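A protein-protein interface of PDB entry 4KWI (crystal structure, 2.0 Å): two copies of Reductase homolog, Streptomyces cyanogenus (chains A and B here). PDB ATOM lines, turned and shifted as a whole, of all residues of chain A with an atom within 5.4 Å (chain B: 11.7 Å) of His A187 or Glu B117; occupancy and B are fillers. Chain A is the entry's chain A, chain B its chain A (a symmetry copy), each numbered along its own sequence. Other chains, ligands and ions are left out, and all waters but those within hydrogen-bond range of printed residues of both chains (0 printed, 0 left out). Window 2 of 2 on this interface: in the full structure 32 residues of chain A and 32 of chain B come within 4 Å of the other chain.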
ATOM      1  N   GLN A 140      -5.771 -23.683 -21.109  1.00  0.00           N
ATOM      2  CA  GLN A 140      -4.888 -22.732 -20.406  1.00  0.00           C
ATOM      3  C   GLN A 140      -4.692 -23.095 -18.922  1.00  0.00           C
ATOM      4  O   GLN A 140      -3.575 -23.092 -18.400  1.00  0.00           O
ATOM      5  CB  GLN A 140      -5.425 -21.289 -20.545  1.00  0.00           C
ATOM      6  CG  GLN A 140      -4.569 -20.230 -19.880  1.00  0.00           C
ATOM      7  CD  GLN A 140      -5.276 -18.891 -19.757  1.00  0.00           C
ATOM      8  OE1 GLN A 140      -6.226 -18.742 -18.986  1.00  0.00           O
ATOM      9  NE2 GLN A 140      -4.798 -17.897 -20.503  1.00  0.00           N
ATOM     10  N   LEU A 143      -2.659 -26.431 -18.343  1.00  0.00           N
ATOM     11  CA  LEU A 143      -1.199 -26.288 -18.433  1.00  0.00           C
ATOM     12  C   LEU A 143      -0.486 -26.241 -17.086  1.00  0.00           C
ATOM     13  O   LEU A 143       0.629 -26.731 -16.975  1.00  0.00           O
ATOM     14  CB  LEU A 143      -0.789 -25.073 -19.273  1.00  0.00           C
ATOM     15  CG  LEU A 143      -1.245 -24.960 -20.735  1.00  0.00           C
ATOM     16  CD1 LEU A 143      -0.431 -23.898 -21.459  1.00  0.00           C
ATOM     17  CD2 LEU A 143      -1.163 -26.275 -21.487  1.00  0.00           C
ATOM     18  N   HIS A 183      -1.403 -24.208 -32.685  1.00  0.00           N
ATOM     19  CA  HIS A 183      -0.528 -23.285 -31.972  1.00  0.00           C
ATOM     20  C   HIS A 183       0.032 -23.812 -30.675  1.00  0.00           C
ATOM     21  O   HIS A 183       1.201 -23.577 -30.377  1.00  0.00           O
ATOM     22  CB  HIS A 183      -1.223 -21.926 -31.766  1.00  0.00           C
ATOM     23  CG  HIS A 183      -1.581 -21.234 -33.060  1.00  0.00           C
ATOM     24  ND1 HIS A 183      -0.686 -20.558 -33.785  1.00  0.00           N
ATOM     25  CD2 HIS A 183      -2.796 -21.152 -33.757  1.00  0.00           C
ATOM     26  CE1 HIS A 183      -1.277 -20.059 -34.891  1.00  0.00           C
ATOM     27  NE2 HIS A 183      -2.569 -20.436 -34.879  1.00  0.00           N
ATOM     28  N   PHE A 184      -0.783 -24.516 -29.889  1.00  0.00           N
ATOM     29  CA  PHE A 184      -0.290 -25.138 -28.641  1.00  0.00           C
ATOM     30  C   PHE A 184       0.662 -26.329 -28.853  1.00  0.00           C
ATOM     31  O   PHE A 184       1.492 -26.635 -27.974  1.00  0.00           O
ATOM     32  CB  PHE A 184      -1.444 -25.532 -27.708  1.00  0.00           C
ATOM     33  CG  PHE A 184      -1.954 -24.390 -26.862  1.00  0.00           C
ATOM     34  CD1 PHE A 184      -1.310 -24.035 -25.679  1.00  0.00           C
ATOM     35  CD2 PHE A 184      -3.074 -23.653 -27.261  1.00  0.00           C
ATOM     36  CE1 PHE A 184      -1.790 -22.984 -24.896  1.00  0.00           C
ATOM     37  CE2 PHE A 184      -3.548 -22.604 -26.487  1.00  0.00           C
ATOM     38  CZ  PHE A 184      -2.904 -22.266 -25.302  1.00  0.00           C
ATOM     39  N   SER A 185       0.569 -26.999 -30.000  1.00  0.00           N
ATOM     40  CA  SER A 185       1.531 -28.069 -30.276  1.00  0.00           C
ATOM     41  C   SER A 185       2.974 -27.523 -30.252  1.00  0.00           C
ATOM     42  O   SER A 185       3.849 -28.121 -29.626  1.00  0.00           O
ATOM     43  CB  SER A 185       1.230 -28.785 -31.596  1.00  0.00           C
ATOM     44  OG  SER A 185       1.405 -27.913 -32.701  1.00  0.00           O
ATOM     45  N   ARG A 186       3.197 -26.388 -30.920  1.00  0.00           N
ATOM     46  CA  ARG A 186       4.483 -25.694 -30.909  1.00  0.00           C
ATOM     47  C   ARG A 186       4.888 -25.206 -29.514  1.00  0.00           C
ATOM     48  O   ARG A 186       6.027 -25.362 -29.117  1.00  0.00           O
ATOM     49  CB  ARG A 186       4.474 -24.520 -31.909  1.00  0.00           C
ATOM     50  CG  ARG A 186       5.788 -23.737 -31.975  1.00  0.00           C
ATOM     51  CD  ARG A 186       5.967 -23.059 -33.336  1.00  0.00           C
ATOM     52  NE  ARG A 186       6.418 -23.993 -34.384  1.00  0.00           N
ATOM     53  CZ  ARG A 186       6.361 -23.773 -35.699  1.00  0.00           C
ATOM     54  NH1 ARG A 186       5.851 -22.643 -36.195  1.00  0.00           N
ATOM     55  NH2 ARG A 186       6.838 -24.696 -36.536  1.00  0.00           N
ATOM     56  N   HIS A 187       3.949 -24.607 -28.792  1.00  0.00           N
ATOM     57  CA  HIS A 187       4.163 -24.162 -27.420  1.00  0.00           C
ATOM     58  C   HIS A 187       4.591 -25.297 -26.504  1.00  0.00           C
ATOM     59  O   HIS A 187       5.536 -25.157 -25.729  1.00  0.00           O
ATOM     60  CB  HIS A 187       2.890 -23.504 -26.887  1.00  0.00           C
ATOM     61  CG  HIS A 187       3.112 -22.637 -25.679  1.00  0.00           C
ATOM     62  ND1 HIS A 187       4.049 -21.663 -25.646  1.00  0.00           N
ATOM     63  CD2 HIS A 187       2.463 -22.599 -24.446  1.00  0.00           C
ATOM     64  CE1 HIS A 187       4.013 -21.044 -24.451  1.00  0.00           C
ATOM     65  NE2 HIS A 187       3.046 -21.615 -23.715  1.00  0.00           N
ATOM     66  N   LEU A 188       3.921 -26.441 -26.616  1.00  0.00           N
ATOM     67  CA  LEU A 188       4.105 -27.527 -25.649  1.00  0.00           C
ATOM     68  C   LEU A 188       5.063 -28.633 -26.105  1.00  0.00           C
ATOM     69  O   LEU A 188       5.105 -29.706 -25.495  1.00  0.00           O
ATOM     70  CB  LEU A 188       2.739 -28.119 -25.242  1.00  0.00           C
ATOM     71  CG  LEU A 188       1.693 -27.134 -24.702  1.00  0.00           C
ATOM     72  CD1 LEU A 188       0.310 -27.777 -24.617  1.00  0.00           C
ATOM     73  CD2 LEU A 188       2.094 -26.528 -23.367  1.00  0.00           C
ATOM     74  N   GLY A 189       5.828 -28.365 -27.161  1.00  0.00           N
ATOM     75  CA  GLY A 189       6.734 -29.357 -27.739  1.00  0.00           C
ATOM     76  C   GLY A 189       7.791 -29.863 -26.777  1.00  0.00           C
ATOM     77  O   GLY A 189       8.031 -31.069 -26.697  1.00  0.00           O
ATOM     78  N   SER A 190       8.422 -28.947 -26.040  1.00  0.00           N
ATOM     79  CA  SER A 190       9.519 -29.312 -25.124  1.00  0.00           C
ATOM     80  C   SER A 190       9.038 -29.977 -23.816  1.00  0.00           C
ATOM     81  O   SER A 190       9.858 -30.463 -23.018  1.00  0.00           O
ATOM     82  CB  SER A 190      10.425 -28.113 -24.827  1.00  0.00           C
ATOM     83  OG  SER A 190       9.847 -27.267 -23.847  1.00  0.00           O
ATOM     84  N   ALA B 112      -3.331  -8.798 -30.773  1.00  0.00           N
ATOM     85  CA  ALA B 112      -2.793  -8.572 -29.425  1.00  0.00           C
ATOM     86  C   ALA B 112      -1.851  -9.697 -28.991  1.00  0.00           C
ATOM     87  O   ALA B 112      -2.254 -10.616 -28.282  1.00  0.00           O
ATOM     88  CB  ALA B 112      -3.917  -8.377 -28.415  1.00  0.00           C
ATOM     89  N   MET B 113      -0.591  -9.599 -29.420  1.00  0.00           N
ATOM     90  CA  MET B 113       0.442 -10.617 -29.170  1.00  0.00           C
ATOM     91  C   MET B 113       0.852 -10.735 -27.696  1.00  0.00           C
ATOM     92  O   MET B 113       0.929  -9.734 -26.987  1.00  0.00           O
ATOM     93  CB  MET B 113       1.662 -10.315 -30.047  1.00  0.00           C
ATOM     94  CG  MET B 113       2.916 -11.107 -29.720  1.00  0.00           C
ATOM     95  SD  MET B 113       4.263 -10.612 -30.803  1.00  0.00           S
ATOM     96  CE  MET B 113       4.969  -9.229 -29.894  1.00  0.00           C
ATOM     97  N   GLY B 114       1.122 -11.961 -27.252  1.00  0.00           N
ATOM     98  CA  GLY B 114       1.446 -12.225 -25.855  1.00  0.00           C
ATOM     99  C   GLY B 114       1.374 -13.697 -25.476  1.00  0.00           C
ATOM    100  O   GLY B 114       0.720 -14.491 -26.146  1.00  0.00           O
ATOM    101  N   ALA B 115       2.056 -14.056 -24.392  1.00  0.00           N
ATOM    102  CA  ALA B 115       2.079 -15.432 -23.898  1.00  0.00           C
ATOM    103  C   ALA B 115       0.641 -15.955 -23.710  1.00  0.00           C
ATOM    104  O   ALA B 115      -0.229 -15.209 -23.262  1.00  0.00           O
ATOM    105  CB  ALA B 115       2.862 -15.502 -22.596  1.00  0.00           C
ATOM    106  N   PRO B 116       0.378 -17.219 -24.085  1.00  0.00           N
ATOM    107  CA  PRO B 116      -1.002 -17.736 -23.957  1.00  0.00           C
ATOM    108  C   PRO B 116      -1.493 -17.900 -22.506  1.00  0.00           C
ATOM    109  O   PRO B 116      -2.698 -17.805 -22.252  1.00  0.00           O
ATOM    110  CB  PRO B 116      -0.958 -19.084 -24.678  1.00  0.00           C
ATOM    111  CG  PRO B 116       0.484 -19.410 -24.844  1.00  0.00           C
ATOM    112  CD  PRO B 116       1.244 -18.126 -24.854  1.00  0.00           C
ATOM    113  N   GLU B 117      -0.563 -18.120 -21.573  1.00  0.00           N
ATOM    114  CA  GLU B 117      -0.886 -18.202 -20.151  1.00  0.00           C
ATOM    115  C   GLU B 117      -1.495 -16.897 -19.628  1.00  0.00           C
ATOM    116  O   GLU B 117      -2.108 -16.882 -18.571  1.00  0.00           O
ATOM    117  CB  GLU B 117       0.362 -18.563 -19.330  1.00  0.00           C
ATOM    118  CG  GLU B 117       0.971 -19.938 -19.624  1.00  0.00           C
ATOM    119  CD  GLU B 117       1.940 -19.965 -20.810  1.00  0.00           C
ATOM    120  OE1 GLU B 117       2.110 -18.935 -21.505  1.00  0.00           O
ATOM    121  OE2 GLU B 117       2.553 -21.032 -21.046  1.00  0.00           O
ATOM    122  N   GLU B 118      -1.342 -15.809 -20.379  1.00  0.00           N
ATOM    123  CA  GLU B 118      -1.731 -14.481 -19.891  1.00  0.00           C
ATOM    124  C   GLU B 118      -3.013 -13.928 -20.515  1.00  0.00           C
ATOM    125  O   GLU B 118      -3.515 -12.887 -20.088  1.00  0.00           O
ATOM    126  CB  GLU B 118      -0.573 -13.502 -20.048  1.00  0.00           C
ATOM    127  CG  GLU B 118       0.722 -14.074 -19.488  1.00  0.00           C
ATOM    128  CD  GLU B 118       1.713 -13.018 -19.056  1.00  0.00           C
ATOM    129  OE1 GLU B 118       1.590 -11.850 -19.496  1.00  0.00           O
ATOM    130  OE2 GLU B 118       2.627 -13.368 -18.274  1.00  0.00           O
ATOM    131  N   VAL B 119      -3.540 -14.636 -21.509  1.00  0.00           N
ATOM    132  CA  VAL B 119      -4.816 -14.281 -22.146  1.00  0.00           C
ATOM    133  C   VAL B 119      -5.970 -14.298 -21.140  1.00  0.00           C
ATOM    134  O   VAL B 119      -6.242 -15.330 -20.512  1.00  0.00           O
ATOM    135  CB  VAL B 119      -5.136 -15.221 -23.329  1.00  0.00           C
ATOM    136  CG1 VAL B 119      -6.507 -14.901 -23.920  1.00  0.00           C
ATOM    137  CG2 VAL B 119      -4.057 -15.111 -24.405  1.00  0.00           C
ATOM    138  N   THR B 120      -6.624 -13.146 -20.981  1.00  0.00           N
ATOM    139  CA  THR B 120      -7.827 -13.027 -20.153  1.00  0.00           C
ATOM    140  C   THR B 120      -9.068 -13.333 -20.992  1.00  0.00           C
ATOM    141  O   THR B 120      -9.008 -13.282 -22.217  1.00  0.00           O
ATOM    142  CB  THR B 120      -7.986 -11.605 -19.556  1.00  0.00           C
ATOM    143  OG1 THR B 120      -8.338 -10.681 -20.595  1.00  0.00           O
ATOM    144  CG2 THR B 120      -6.702 -11.148 -18.854  1.00  0.00           C
ATOM    145  N   PRO B 121     -10.202 -13.652 -20.338  1.00  0.00           N
ATOM    146  CA  PRO B 121     -11.437 -13.847 -21.109  1.00  0.00           C
ATOM    147  C   PRO B 121     -11.865 -12.607 -21.886  1.00  0.00           C
ATOM    148  O   PRO B 121     -12.456 -12.731 -22.953  1.00  0.00           O
ATOM    149  CB  PRO B 121     -12.477 -14.177 -20.033  1.00  0.00           C
ATOM    150  CG  PRO B 121     -11.685 -14.766 -18.919  1.00  0.00           C
ATOM    151  CD  PRO B 121     -10.363 -14.052 -18.923  1.00  0.00           C
ATOM    152  N   GLU B 122     -11.580 -11.422 -21.344  1.00  0.00           N
ATOM    153  CA  GLU B 122     -11.982 -10.171 -21.995  1.00  0.00           C
ATOM    154  C   GLU B 122     -11.173  -9.939 -23.264  1.00  0.00           C
ATOM    155  O   GLU B 122     -11.687  -9.383 -24.240  1.00  0.00           O
ATOM    156  CB  GLU B 122     -11.855  -8.968 -21.044  1.00  0.00           C
ATOM    157  CG  GLU B 122     -12.819  -8.986 -19.860  1.00  0.00           C
ATOM    158  CD  GLU B 122     -12.620 -10.185 -18.929  1.00  0.00           C
ATOM    159  OE1 GLU B 122     -11.466 -10.460 -18.508  1.00  0.00           O
ATOM    160  OE2 GLU B 122     -13.630 -10.869 -18.624  1.00  0.00           O
ATOM    161  N   MET B 123      -9.904 -10.337 -23.236  1.00  0.00           N
ATOM    162  CA  MET B 123      -9.041 -10.230 -24.412  1.00  0.00           C
ATOM    163  C   MET B 123      -9.539 -11.157 -25.513  1.00  0.00           C
ATOM    164  O   MET B 123      -9.550 -10.795 -26.692  1.00  0.00           O
ATOM    165  CB  MET B 123      -7.594 -10.571 -24.062  1.00  0.00           C
ATOM    166  CG  MET B 123      -6.910  -9.564 -23.151  1.00  0.00           C
ATOM    167  SD  MET B 123      -5.346 -10.221 -22.556  1.00  0.00           S
ATOM    168  CE  MET B 123      -4.402 -10.344 -24.078  1.00  0.00           C
ATOM    169  N   PHE B 124      -9.951 -12.353 -25.106  1.00  0.00           N
ATOM    170  CA  PHE B 124     -10.510 -13.348 -26.004  1.00  0.00           C
ATOM    171  C   PHE B 124     -11.818 -12.855 -26.653  1.00  0.00           C
ATOM    172  O   PHE B 124     -12.001 -13.008 -27.860  1.00  0.00           O
ATOM    173  CB  PHE B 124     -10.732 -14.681 -25.258  1.00  0.00           C
ATOM    174  CG  PHE B 124     -11.153 -15.809 -26.156  1.00  0.00           C
ATOM    175  CD1 PHE B 124     -12.473 -15.893 -26.627  1.00  0.00           C
ATOM    176  CD2 PHE B 124     -10.236 -16.775 -26.559  1.00  0.00           C
ATOM    177  CE1 PHE B 124     -12.855 -16.911 -27.488  1.00  0.00           C
ATOM    178  CE2 PHE B 124     -10.619 -17.800 -27.405  1.00  0.00           C
ATOM    179  CZ  PHE B 124     -11.931 -17.873 -27.873  1.00  0.00           C
ATOM    180  N   VAL B 162       0.521 -21.276 -39.830  1.00  0.00           N
ATOM    181  CA  VAL B 162       1.845 -21.253 -39.180  1.00  0.00           C
ATOM    182  C   VAL B 162       1.674 -21.112 -37.660  1.00  0.00           C
ATOM    183  O   VAL B 162       1.154 -20.099 -37.179  1.00  0.00           O
ATOM    184  CB  VAL B 162       2.739 -20.102 -39.719  1.00  0.00           C
ATOM    185  CG1 VAL B 162       4.116 -20.102 -39.051  1.00  0.00           C
ATOM    186  CG2 VAL B 162       2.906 -20.205 -41.234  1.00  0.00           C
ATOM    187  N   ALA B 163       2.112 -22.122 -36.913  1.00  0.00           N
ATOM    188  CA  ALA B 163       1.971 -22.136 -35.460  1.00  0.00           C
ATOM    189  C   ALA B 163       2.797 -21.035 -34.791  1.00  0.00           C
ATOM    190  O   ALA B 163       3.994 -20.933 -35.043  1.00  0.00           O
ATOM    191  CB  ALA B 163       2.379 -23.503 -34.918  1.00  0.00           C
ATOM    192  N   SER B 164       2.147 -20.209 -33.965  1.00  0.00           N
ATOM    193  CA  SER B 164       2.821 -19.196 -33.133  1.00  0.00           C
ATOM    194  C   SER B 164       2.052 -19.038 -31.821  1.00  0.00           C
ATOM    195  O   SER B 164       0.968 -18.437 -31.805  1.00  0.00           O
ATOM    196  CB  SER B 164       2.920 -17.837 -33.841  1.00  0.00           C
ATOM    197  OG  SER B 164       3.342 -17.989 -35.187  1.00  0.00           O
ATOM    198  N   PRO B 165       2.591 -19.599 -30.724  1.00  0.00           N
ATOM    199  CA  PRO B 165       1.976 -19.543 -29.400  1.00  0.00           C
ATOM    200  C   PRO B 165       1.502 -18.140 -29.009  1.00  0.00           C
ATOM    201  O   PRO B 165       0.416 -17.992 -28.433  1.00  0.00           O
ATOM    202  CB  PRO B 165       3.115 -19.993 -28.482  1.00  0.00           C
ATOM    203  CG  PRO B 165       3.898 -20.943 -29.316  1.00  0.00           C
ATOM    204  CD  PRO B 165       3.791 -20.458 -30.734  1.00  0.00           C
ATOM    205  N   ASP B 166       2.298 -17.123 -29.346  1.00  0.00           N
ATOM    206  CA  ASP B 166       1.995 -15.723 -29.003  1.00  0.00           C
ATOM    207  C   ASP B 166       0.768 -15.158 -29.716  1.00  0.00           C
ATOM    208  O   ASP B 166       0.285 -14.074 -29.366  1.00  0.00           O
ATOM    209  CB  ASP B 166       3.198 -14.823 -29.299  1.00  0.00           C
ATOM    210  CG  ASP B 166       4.289 -14.922 -28.251  1.00  0.00           C
ATOM    211  OD1 ASP B 166       4.098 -15.593 -27.207  1.00  0.00           O
ATOM    212  OD2 ASP B 166       5.356 -14.295 -28.471  1.00  0.00           O
ATOM    213  N   GLN B 167       0.280 -15.887 -30.716  1.00  0.00           N
ATOM    214  CA  GLN B 167      -0.794 -15.411 -31.581  1.00  0.00           C
ATOM    215  C   GLN B 167      -2.010 -16.336 -31.585  1.00  0.00           C
ATOM    216  O   GLN B 167      -2.867 -16.234 -32.478  1.00  0.00           O
ATOM    217  CB  GLN B 167      -0.279 -15.265 -33.021  1.00  0.00           C
ATOM    218  CG  GLN B 167       0.924 -14.344 -33.212  1.00  0.00           C
ATOM    219  CD  GLN B 167       0.550 -12.874 -33.217  1.00  0.00           C
ATOM    220  OE1 GLN B 167      -0.506 -12.489 -32.713  1.00  0.00           O
ATOM    221  NE2 GLN B 167       1.414 -12.042 -33.794  1.00  0.00           N
ATOM    222  N   VAL B 168      -2.103 -17.225 -30.592  1.00  0.00           N
ATOM    223  CA  VAL B 168      -3.132 -18.283 -30.620  1.00  0.00           C
ATOM    224  C   VAL B 168      -4.592 -17.773 -30.694  1.00  0.00           C
ATOM    225  O   VAL B 168      -5.369 -18.276 -31.491  1.00  0.00           O
ATOM    226  CB  VAL B 168      -2.923 -19.359 -29.519  1.00  0.00           C
ATOM    227  CG1 VAL B 168      -2.929 -18.751 -28.124  1.00  0.00           C
ATOM    228  CG2 VAL B 168      -3.971 -20.468 -29.640  1.00  0.00           C
ATOM    229  N   THR B 169      -4.957 -16.774 -29.888  1.00  0.00           N
ATOM    230  CA  THR B 169      -6.324 -16.233 -29.947  1.00  0.00           C
ATOM    231  C   THR B 169      -6.578 -15.472 -31.252  1.00  0.00           C
ATOM    232  O   THR B 169      -7.679 -15.501 -31.799  1.00  0.00           O
ATOM    233  CB  THR B 169      -6.668 -15.333 -28.735  1.00  0.00           C
ATOM    234  OG1 THR B 169      -5.810 -14.188 -28.724  1.00  0.00           O
ATOM    235  CG2 THR B 169      -6.515 -16.105 -27.418  1.00  0.00           C
ATOM    236  N   MET B 172      -7.169 -18.377 -33.642  1.00  0.00           N
ATOM    237  CA  MET B 172      -8.533 -18.878 -33.463  1.00  0.00           C
ATOM    238  C   MET B 172      -9.591 -18.009 -34.165  1.00  0.00           C
ATOM    239  O   MET B 172     -10.463 -18.543 -34.851  1.00  0.00           O
ATOM    240  CB  MET B 172      -8.884 -19.056 -31.971  1.00  0.00           C
ATOM    241  CG  MET B 172      -8.102 -20.155 -31.254  1.00  0.00           C
ATOM    242  SD  MET B 172      -8.563 -20.315 -29.509  1.00  0.00           S
ATOM    243  CE  MET B 172     -10.245 -20.949 -29.654  1.00  0.00           C
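The backbone carbonyl oxygen of Pro B116 sits at hydrogen-bond distance from the side-chain amide nitrogen of Gln A140. The backbone carbonyl oxygen of Glu B117 lies within hydrogen-bond range of the side-chain amide nitrogen of Gln A140, 3.5 Å away. The backbone carbonyl oxygen (O) of Val B119 sits at hydrogen-bond distance from the side-chain amide nitrogen (NE2) of Gln A140. A ring nitrogen (ND1) of His A183 sits at hydrogen-bond distance from the backbone NH (N) of Ser B164. The guanidinium group (NH1) of Arg A186 is in hydrogen-bond range of the backbone carbonyl oxygen (O) of Ala B163. OE2 of Glu B117 sits at hydrogen-bond distance from NE2 of His A187, at 2.8 Å.
Val B162 touches His A183 (O to CE1, 3.3 Å). CA of Ala B163 touches ND1 of His A183, at 3.5 Å. Pro B165 touches His A183. CB of His A183 touches CG2 of Val B168, 3.8 Å away. Pro B116 touches Phe A184. Val B168 touches Phe A184 (CG2 to CE2, 3.8 Å). His A187 touches Pro B116. Pro B165 touches His A187.
His A187 touches just these residues of chain B: Pro B116 (3.6 Å), Glu B117 (2.8 Å) and Pro B165 (3.4 Å). Glu B117 touches two residues of chain A. Of chain B, only Pro B116 (2.7 Å), Glu B117 (3.5 Å) and Val B119 (2.9 Å) come within 4 Å of Gln A140. No residue of chain B comes within 4 Å of Leu A143. Ser A185 touches none of the printed residues of chain B. No residue of chain B comes within 4 Å of Leu A188. Gly A189 touches none of the printed residues of chain B. Ser A190 touches none of the printed residues of chain B. Of the printed residues of chain A, Ser B164 touches His A183 (2.9 Å). Printed residues of chain A within 4 Å of Val B168: His A183 and Phe A184. Of the printed residues of chain A, Val B119 touches Gln A140 (2.9 Å). Printed residues of chain A within 4 Å of Ala B163: His A183 and Arg A186. Printed residues of chain A within 4 Å of Val B162: His A183 (3.3 Å). The nearest residue of chain B that does not touch His A187 is Ala B115 (6.0 Å). The nearest residue of chain A that does not touch Glu B117 is Leu A143 (4.2 Å).
Along chain B the printed residues that touch a printed residue of chain A span positions 116 to 168. Among the printed residues, no Asp or Glu carboxylate lies within 4 Å of a Lys or Arg side-chain nitrogen of the other chain.
No position is printed for both chains. Of the 14 pairs that touch across the chains among the printed residues, none has its exchanged pair printed and touching as well.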
